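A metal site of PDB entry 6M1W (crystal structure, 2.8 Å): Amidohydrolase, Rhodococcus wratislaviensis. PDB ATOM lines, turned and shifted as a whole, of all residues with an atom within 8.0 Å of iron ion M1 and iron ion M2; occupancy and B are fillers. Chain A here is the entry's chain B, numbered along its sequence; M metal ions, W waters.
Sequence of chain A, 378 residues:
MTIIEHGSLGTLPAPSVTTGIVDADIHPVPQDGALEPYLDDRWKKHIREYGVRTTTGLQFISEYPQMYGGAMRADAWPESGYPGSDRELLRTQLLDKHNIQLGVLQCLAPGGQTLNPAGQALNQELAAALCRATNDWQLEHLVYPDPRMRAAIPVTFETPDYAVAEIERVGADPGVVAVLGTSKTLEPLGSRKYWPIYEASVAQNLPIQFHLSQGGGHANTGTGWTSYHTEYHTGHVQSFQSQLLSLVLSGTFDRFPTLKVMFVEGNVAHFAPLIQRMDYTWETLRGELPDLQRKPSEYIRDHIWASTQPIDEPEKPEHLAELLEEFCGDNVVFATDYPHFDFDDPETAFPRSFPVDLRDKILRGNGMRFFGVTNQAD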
ATOM      1  N   ALA A  24      -8.950 -16.099  14.709  1.00  0.00           N
ATOM      2  CA  ALA A  24     -10.351 -16.324  14.466  1.00  0.00           C
ATOM      3  C   ALA A  24     -11.210 -15.094  14.776  1.00  0.00           C
ATOM      4  O   ALA A  24     -12.436 -15.206  14.695  1.00  0.00           O
ATOM      5  CB  ALA A  24     -10.827 -17.539  15.275  1.00  0.00           C
ATOM      6  N   ASP A  25     -10.629 -13.939  15.096  1.00  0.00           N
ATOM      7  CA  ASP A  25     -11.441 -12.760  15.420  1.00  0.00           C
ATOM      8  C   ASP A  25     -10.689 -11.488  15.040  1.00  0.00           C
ATOM      9  O   ASP A  25      -9.872 -10.971  15.827  1.00  0.00           O
ATOM     10  CB  ASP A  25     -11.816 -12.764  16.896  1.00  0.00           C
ATOM     11  CG  ASP A  25     -13.088 -12.005  17.170  1.00  0.00           C
ATOM     12  OD1 ASP A  25     -14.061 -12.165  16.409  1.00  0.00           O
ATOM     13  OD2 ASP A  25     -13.141 -11.291  18.186  1.00  0.00           O
ATOM     14  N   ILE A  26     -10.989 -10.971  13.848  1.00  0.00           N
ATOM     15  CA  ILE A  26     -10.531  -9.666  13.370  1.00  0.00           C
ATOM     16  C   ILE A  26     -11.739  -8.773  13.165  1.00  0.00           C
ATOM     17  O   ILE A  26     -12.674  -9.169  12.458  1.00  0.00           O
ATOM     18  CB  ILE A  26      -9.775  -9.779  12.033  1.00  0.00           C
ATOM     19  CG1 ILE A  26      -8.552 -10.696  12.158  1.00  0.00           C
ATOM     20  CG2 ILE A  26      -9.485  -8.383  11.483  1.00  0.00           C
ATOM     21  CD1 ILE A  26      -7.319 -10.054  12.707  1.00  0.00           C
ATOM     22  N   HIS A  27     -11.704  -7.569  13.737  1.00  0.00           N
ATOM     23  CA  HIS A  27     -12.807  -6.626  13.563  1.00  0.00           C
ATOM     24  C   HIS A  27     -12.445  -5.504  12.609  1.00  0.00           C
ATOM     25  O   HIS A  27     -11.830  -4.516  13.023  1.00  0.00           O
ATOM     26  CB  HIS A  27     -13.242  -6.042  14.910  1.00  0.00           C
ATOM     27  CG  HIS A  27     -13.889  -7.034  15.814  1.00  0.00           C
ATOM     28  ND1 HIS A  27     -14.998  -7.764  15.456  1.00  0.00           N
ATOM     29  CD2 HIS A  27     -13.586  -7.406  17.073  1.00  0.00           C
ATOM     30  CE1 HIS A  27     -15.347  -8.561  16.452  1.00  0.00           C
ATOM     31  NE2 HIS A  27     -14.500  -8.364  17.446  1.00  0.00           N
ATOM     32  N   GLN A  66     -19.315   1.104  26.597  1.00  0.00           N
ATOM     33  CA  GLN A  66     -17.849   1.190  26.707  1.00  0.00           C
ATOM     34  C   GLN A  66     -17.440   2.152  27.816  1.00  0.00           C
ATOM     35  O   GLN A  66     -16.301   2.157  28.281  1.00  0.00           O
ATOM     36  CB  GLN A  66     -17.207   1.638  25.390  1.00  0.00           C
ATOM     37  CG  GLN A  66     -16.754   0.558  24.424  1.00  0.00           C
ATOM     38  CD  GLN A  66     -15.428  -0.040  24.782  1.00  0.00           C
ATOM     39  OE1 GLN A  66     -15.272  -0.665  25.842  1.00  0.00           O
ATOM     40  NE2 GLN A  66     -14.448   0.157  23.907  1.00  0.00           N
ATOM     41  N   GLN A 106     -15.005 -10.549  11.381  1.00  0.00           N
ATOM     42  CA  GLN A 106     -16.217 -10.549  12.185  1.00  0.00           C
ATOM     43  C   GLN A 106     -16.642  -9.101  12.296  1.00  0.00           C
ATOM     44  O   GLN A 106     -16.267  -8.400  13.235  1.00  0.00           O
ATOM     45  CB  GLN A 106     -15.946 -11.200  13.540  1.00  0.00           C
ATOM     46  CG  GLN A 106     -15.361 -12.602  13.378  1.00  0.00           C
ATOM     47  CD  GLN A 106     -15.883 -13.617  14.388  1.00  0.00           C
ATOM     48  OE1 GLN A 106     -16.910 -13.408  15.043  1.00  0.00           O
ATOM     49  NE2 GLN A 106     -15.197 -14.742  14.484  1.00  0.00           N
ATOM     50  N   LEU A 108     -19.356  -6.623  13.227  1.00  0.00           N
ATOM     51  CA  LEU A 108     -20.635  -6.452  13.903  1.00  0.00           C
ATOM     52  C   LEU A 108     -21.619  -5.709  13.000  1.00  0.00           C
ATOM     53  O   LEU A 108     -22.621  -6.277  12.549  1.00  0.00           O
ATOM     54  CB  LEU A 108     -20.439  -5.714  15.231  1.00  0.00           C
ATOM     55  CG  LEU A 108     -19.558  -6.442  16.252  1.00  0.00           C
ATOM     56  CD1 LEU A 108     -19.776  -7.963  16.218  1.00  0.00           C
ATOM     57  CD2 LEU A 108     -18.079  -6.079  16.083  1.00  0.00           C
ATOM     58  N   HIS A 211     -20.345 -14.802  18.369  1.00  0.00           N
ATOM     59  CA  HIS A 211     -19.471 -13.797  18.924  1.00  0.00           C
ATOM     60  C   HIS A 211     -20.187 -13.028  20.037  1.00  0.00           C
ATOM     61  O   HIS A 211     -21.377 -12.688  19.898  1.00  0.00           O
ATOM     62  CB  HIS A 211     -19.026 -12.834  17.822  1.00  0.00           C
ATOM     63  CG  HIS A 211     -17.979 -11.861  18.253  1.00  0.00           C
ATOM     64  ND1 HIS A 211     -18.250 -10.763  19.042  1.00  0.00           N
ATOM     65  CD2 HIS A 211     -16.645 -11.806  17.986  1.00  0.00           C
ATOM     66  CE1 HIS A 211     -17.143 -10.092  19.259  1.00  0.00           C
ATOM     67  NE2 HIS A 211     -16.151 -10.705  18.623  1.00  0.00           N
ATOM     68  N   LEU A 212     -19.431 -12.741  21.102  1.00  0.00           N
ATOM     69  CA  LEU A 212     -19.895 -11.988  22.260  1.00  0.00           C
ATOM     70  C   LEU A 212     -20.787 -10.836  21.842  1.00  0.00           C
ATOM     71  O   LEU A 212     -20.516 -10.157  20.840  1.00  0.00           O
ATOM     72  CB  LEU A 212     -18.678 -11.478  23.039  1.00  0.00           C
ATOM     73  CG  LEU A 212     -18.754 -10.369  24.094  1.00  0.00           C
ATOM     74  CD1 LEU A 212     -17.681 -10.584  25.111  1.00  0.00           C
ATOM     75  CD2 LEU A 212     -18.586  -8.977  23.510  1.00  0.00           C
ATOM     76  N   HIS A 233     -18.775  -6.694  31.741  1.00  0.00           N
ATOM     77  CA  HIS A 233     -17.777  -7.391  30.944  1.00  0.00           C
ATOM     78  C   HIS A 233     -17.626  -8.854  31.366  1.00  0.00           C
ATOM     79  O   HIS A 233     -17.587  -9.749  30.515  1.00  0.00           O
ATOM     80  CB  HIS A 233     -16.423  -6.663  31.014  1.00  0.00           C
ATOM     81  CG  HIS A 233     -15.649  -6.680  29.724  1.00  0.00           C
ATOM     82  ND1 HIS A 233     -15.352  -5.532  29.027  1.00  0.00           N
ATOM     83  CD2 HIS A 233     -15.128  -7.710  29.024  1.00  0.00           C
ATOM     84  CE1 HIS A 233     -14.677  -5.857  27.937  1.00  0.00           C
ATOM     85  NE2 HIS A 233     -14.520  -7.166  27.909  1.00  0.00           N
ATOM     86  N   VAL A 264     -16.739 -17.264  20.658  1.00  0.00           N
ATOM     87  CA  VAL A 264     -15.717 -16.269  20.393  1.00  0.00           C
ATOM     88  C   VAL A 264     -15.843 -15.121  21.394  1.00  0.00           C
ATOM     89  O   VAL A 264     -16.943 -14.667  21.692  1.00  0.00           O
ATOM     90  CB  VAL A 264     -15.817 -15.718  18.954  1.00  0.00           C
ATOM     91  CG1 VAL A 264     -14.643 -14.833  18.669  1.00  0.00           C
ATOM     92  CG2 VAL A 264     -15.901 -16.850  17.949  1.00  0.00           C
ATOM     93  N   GLU A 265     -14.694 -14.645  21.874  1.00  0.00           N
ATOM     94  CA  GLU A 265     -14.565 -13.613  22.909  1.00  0.00           C
ATOM     95  C   GLU A 265     -15.318 -14.030  24.172  1.00  0.00           C
ATOM     96  O   GLU A 265     -15.807 -13.190  24.944  1.00  0.00           O
ATOM     97  CB  GLU A 265     -14.966 -12.223  22.389  1.00  0.00           C
ATOM     98  CG  GLU A 265     -14.613 -11.079  23.350  1.00  0.00           C
ATOM     99  CD  GLU A 265     -14.147  -9.822  22.691  1.00  0.00           C
ATOM    100  OE1 GLU A 265     -14.218  -9.758  21.452  1.00  0.00           O
ATOM    101  OE2 GLU A 265     -13.729  -8.898  23.438  1.00  0.00           O
ATOM    102  N   GLY A 266     -15.469 -15.327  24.385  1.00  0.00           N
ATOM    103  CA  GLY A 266     -16.172 -15.826  25.552  1.00  0.00           C
ATOM    104  C   GLY A 266     -15.359 -16.436  26.672  1.00  0.00           C
ATOM    105  O   GLY A 266     -15.967 -16.867  27.663  1.00  0.00           O
ATOM    106  N   SER A 307     -12.609 -19.611  20.917  1.00  0.00           N
ATOM    107  CA  SER A 307     -11.561 -18.611  20.763  1.00  0.00           C
ATOM    108  C   SER A 307     -10.882 -18.333  22.085  1.00  0.00           C
ATOM    109  O   SER A 307     -11.470 -18.513  23.148  1.00  0.00           O
ATOM    110  CB  SER A 307     -12.151 -17.317  20.188  1.00  0.00           C
ATOM    111  OG  SER A 307     -11.541 -16.115  20.628  1.00  0.00           O
ATOM    112  N   GLN A 309      -9.348 -15.320  23.034  1.00  0.00           N
ATOM    113  CA  GLN A 309      -9.308 -13.952  23.510  1.00  0.00           C
ATOM    114  C   GLN A 309     -10.581 -13.643  24.302  1.00  0.00           C
ATOM    115  O   GLN A 309     -11.663 -14.081  23.911  1.00  0.00           O
ATOM    116  CB  GLN A 309      -9.189 -12.993  22.324  1.00  0.00           C
ATOM    117  CG  GLN A 309      -8.750 -11.601  22.703  1.00  0.00           C
ATOM    118  CD  GLN A 309      -9.930 -10.708  23.054  1.00  0.00           C
ATOM    119  OE1 GLN A 309     -11.002 -10.812  22.443  1.00  0.00           O
ATOM    120  NE2 GLN A 309      -9.743  -9.844  24.042  1.00  0.00           N
ATOM    121  N   PRO A 310     -10.477 -12.935  25.436  1.00  0.00           N
ATOM    122  CA  PRO A 310      -9.225 -12.560  26.104  1.00  0.00           C
ATOM    123  C   PRO A 310      -8.654 -13.724  26.919  1.00  0.00           C
ATOM    124  O   PRO A 310      -9.407 -14.526  27.489  1.00  0.00           O
ATOM    125  CB  PRO A 310      -9.647 -11.409  27.014  1.00  0.00           C
ATOM    126  CG  PRO A 310     -11.093 -11.718  27.358  1.00  0.00           C
ATOM    127  CD  PRO A 310     -11.670 -12.369  26.117  1.00  0.00           C
ATOM    128  N   ALA A 335      -7.095 -16.072  18.871  1.00  0.00           N
ATOM    129  CA  ALA A 335      -7.693 -14.820  18.403  1.00  0.00           C
ATOM    130  C   ALA A 335      -6.963 -13.652  19.050  1.00  0.00           C
ATOM    131  O   ALA A 335      -6.460 -13.772  20.178  1.00  0.00           O
ATOM    132  CB  ALA A 335      -9.186 -14.745  18.724  1.00  0.00           C
ATOM    133  N   THR A 336      -6.891 -12.529  18.318  1.00  0.00           N
ATOM    134  CA  THR A 336      -6.392 -11.262  18.846  1.00  0.00           C
ATOM    135  C   THR A 336      -7.493 -10.321  19.301  1.00  0.00           C
ATOM    136  O   THR A 336      -7.306  -9.622  20.305  1.00  0.00           O
ATOM    137  CB  THR A 336      -5.576 -10.501  17.795  1.00  0.00           C
ATOM    138  OG1 THR A 336      -4.706 -11.395  17.090  1.00  0.00           O
ATOM    139  CG2 THR A 336      -4.749  -9.375  18.435  1.00  0.00           C
ATOM    140  N   ASP A 337      -8.602 -10.261  18.551  1.00  0.00           N
ATOM    141  CA  ASP A 337      -9.530  -9.144  18.644  1.00  0.00           C
ATOM    142  C   ASP A 337      -8.782  -7.849  18.344  1.00  0.00           C
ATOM    143  O   ASP A 337      -8.621  -6.961  19.193  1.00  0.00           O
ATOM    144  CB  ASP A 337     -10.209  -9.114  20.022  1.00  0.00           C
ATOM    145  CG  ASP A 337     -11.685  -8.783  19.972  1.00  0.00           C
ATOM    146  OD1 ASP A 337     -12.335  -9.007  18.941  1.00  0.00           O
ATOM    147  OD2 ASP A 337     -12.184  -8.277  20.964  1.00  0.00           O
ATOM    148  N   TYR A 338      -8.258  -7.794  17.162  1.00  0.00           N
ATOM    149  CA  TYR A 338      -7.863  -6.497  16.625  1.00  0.00           C
ATOM    150  C   TYR A 338      -9.116  -5.759  16.154  1.00  0.00           C
ATOM    151  O   TYR A 338     -10.009  -6.366  15.544  1.00  0.00           O
ATOM    152  CB  TYR A 338      -6.892  -6.679  15.460  1.00  0.00           C
ATOM    153  CG  TYR A 338      -6.118  -5.427  15.125  1.00  0.00           C
ATOM    154  CD1 TYR A 338      -5.130  -4.939  15.972  1.00  0.00           C
ATOM    155  CD2 TYR A 338      -6.377  -4.728  13.950  1.00  0.00           C
ATOM    156  CE1 TYR A 338      -4.421  -3.777  15.660  1.00  0.00           C
ATOM    157  CE2 TYR A 338      -5.679  -3.575  13.621  1.00  0.00           C
ATOM    158  CZ  TYR A 338      -4.691  -3.108  14.492  1.00  0.00           C
ATOM    159  OH  TYR A 338      -3.993  -1.958  14.176  1.00  0.00           O
ATOM    160  N   PRO A 339      -9.210  -4.447  16.408  1.00  0.00           N
ATOM    161  CA  PRO A 339      -8.229  -3.622  17.116  1.00  0.00           C
ATOM    162  C   PRO A 339      -8.585  -3.314  18.571  1.00  0.00           C
ATOM    163  O   PRO A 339      -8.131  -2.303  19.113  1.00  0.00           O
ATOM    164  CB  PRO A 339      -8.221  -2.345  16.289  1.00  0.00           C
ATOM    165  CG  PRO A 339      -9.680  -2.202  15.859  1.00  0.00           C
ATOM    166  CD  PRO A 339     -10.282  -3.606  15.826  1.00  0.00           C
ATOM    167  N   HIS A 340      -9.399  -4.176  19.193  1.00  0.00           N
ATOM    168  CA  HIS A 340      -9.974  -3.878  20.498  1.00  0.00           C
ATOM    169  C   HIS A 340      -8.894  -3.695  21.561  1.00  0.00           C
ATOM    170  O   HIS A 340      -7.767  -4.201  21.454  1.00  0.00           O
ATOM    171  CB  HIS A 340     -10.944  -4.977  20.924  1.00  0.00           C
ATOM    172  CG  HIS A 340     -12.298  -4.901  20.269  1.00  0.00           C
ATOM    173  ND1 HIS A 340     -13.376  -5.639  20.691  1.00  0.00           N
ATOM    174  CD2 HIS A 340     -12.729  -4.174  19.209  1.00  0.00           C
ATOM    175  CE1 HIS A 340     -14.422  -5.368  19.929  1.00  0.00           C
ATOM    176  NE2 HIS A 340     -14.052  -4.480  19.030  1.00  0.00           N
ATOM    177  N   PHE A 341      -9.253  -2.964  22.630  1.00  0.00           N
ATOM    178  CA  PHE A 341      -8.292  -2.571  23.650  1.00  0.00           C
ATOM    179  C   PHE A 341      -7.679  -3.776  24.357  1.00  0.00           C
ATOM    180  O   PHE A 341      -6.521  -3.732  24.774  1.00  0.00           O
ATOM    181  CB  PHE A 341      -8.942  -1.611  24.657  1.00  0.00           C
ATOM    182  CG  PHE A 341      -9.616  -2.290  25.834  1.00  0.00           C
ATOM    183  CD1 PHE A 341      -8.891  -2.583  26.997  1.00  0.00           C
ATOM    184  CD2 PHE A 341     -10.961  -2.603  25.800  1.00  0.00           C
ATOM    185  CE1 PHE A 341      -9.504  -3.195  28.094  1.00  0.00           C
ATOM    186  CE2 PHE A 341     -11.586  -3.220  26.889  1.00  0.00           C
ATOM    187  CZ  PHE A 341     -10.852  -3.518  28.043  1.00  0.00           C
ATOM    188  N   ASP A 342      -8.434  -4.872  24.484  1.00  0.00           N
ATOM    189  CA  ASP A 342      -7.980  -6.059  25.194  1.00  0.00           C
ATOM    190  C   ASP A 342      -7.423  -7.099  24.242  1.00  0.00           C
ATOM    191  O   ASP A 342      -7.620  -8.305  24.430  1.00  0.00           O
ATOM    192  CB  ASP A 342      -9.086  -6.662  26.063  1.00  0.00           C
ATOM    193  CG  ASP A 342     -10.462  -6.735  25.369  1.00  0.00           C
ATOM    194  OD1 ASP A 342     -10.693  -6.046  24.336  1.00  0.00           O
ATOM    195  OD2 ASP A 342     -11.334  -7.478  25.892  1.00  0.00           O
ATOM    196  N   PHE A 343      -6.727  -6.654  23.201  1.00  0.00           N
ATOM    197  CA  PHE A 343      -6.059  -7.542  22.278  1.00  0.00           C
ATOM    198  C   PHE A 343      -4.874  -8.255  22.948  1.00  0.00           C
ATOM    199  O   PHE A 343      -4.281  -7.758  23.906  1.00  0.00           O
ATOM    200  CB  PHE A 343      -5.562  -6.765  21.060  1.00  0.00           C
ATOM    201  CG  PHE A 343      -4.236  -6.121  21.262  1.00  0.00           C
ATOM    202  CD1 PHE A 343      -4.102  -5.074  22.184  1.00  0.00           C
ATOM    203  CD2 PHE A 343      -3.107  -6.580  20.582  1.00  0.00           C
ATOM    204  CE1 PHE A 343      -2.870  -4.482  22.391  1.00  0.00           C
ATOM    205  CE2 PHE A 343      -1.875  -5.988  20.789  1.00  0.00           C
ATOM    206  CZ  PHE A 343      -1.751  -4.937  21.697  1.00  0.00           C
HETATM  207 FE    FE M   1     -13.811  -7.381  21.770  1.00  0.00          FE
HETATM  208 FE    FE M   2     -14.409  -9.767  19.152  1.00  0.00          FE
HETATM  209  O   HOH W   1     -13.807  -5.913  24.095  1.00  0.00           O
HETATM  210  O   HOH W   2     -16.365  -6.412  22.035  1.00  0.00           O
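Of the 25 residues printed, 5 come within 4 Å of iron ion M2. The nearest printed residue that does not touch iron ion M2 is His 340 (4.5 Å).
The backbone NH (N) of His 27 lies within hydrogen-bond range of the backbone carbonyl oxygen (O) of Tyr 338 (2.8 Å). The side-chain amide oxygen (OE1) of Gln 309 sits close to the side-chain carboxylate (OD2) of Asp 337 (3.2 Å). ND1 of His 27 lies within hydrogen-bond range of O of Gln 106 (2.6 Å). OE1 of Gln 309 lies close to OE2 of Glu 265. The side-chain carboxylate (OD1) of Asp 25 lies close to the side-chain amide oxygen (OE1) of Gln 106 (3.4 Å).
Iron ion M2 is bound by a ring nitrogen (NE2) of His 211 (2.0 Å), the side-chain carboxylate of Asp 25 (2.2 Å), a ring nitrogen (NE2) of His 27 (2.2 Å), the side-chain carboxylate of Asp 337 (2.2 Å) and the side-chain carboxylate of Glu 265 (2.3 Å). Iron ion M2 has five donor atoms within binding distance.
Within 4 Å of iron ion M1: Glu 265, Asp 337 and His 340. Along chain A the residues within 4 Å of iron ion M1 span positions 265 to 340.
The side-chain carboxylate (OD2) of Asp 337 binds iron ion M1. ND1 of His 340 is bound to iron ion M1, 2.1 Å away. Iron ion M1 is bound by the side-chain carboxylate (OE2) of Glu 265 (2.3 Å). Iron ion M1 is bound by OE1 of Glu 265 (2.4 Å). Iron ion M1 has four donor atoms within binding distance. Slightly farther from iron ion M1 lies water W2 (2.7 Å). Slightly farther from iron ion M1 lies water W1 (2.7 Å).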
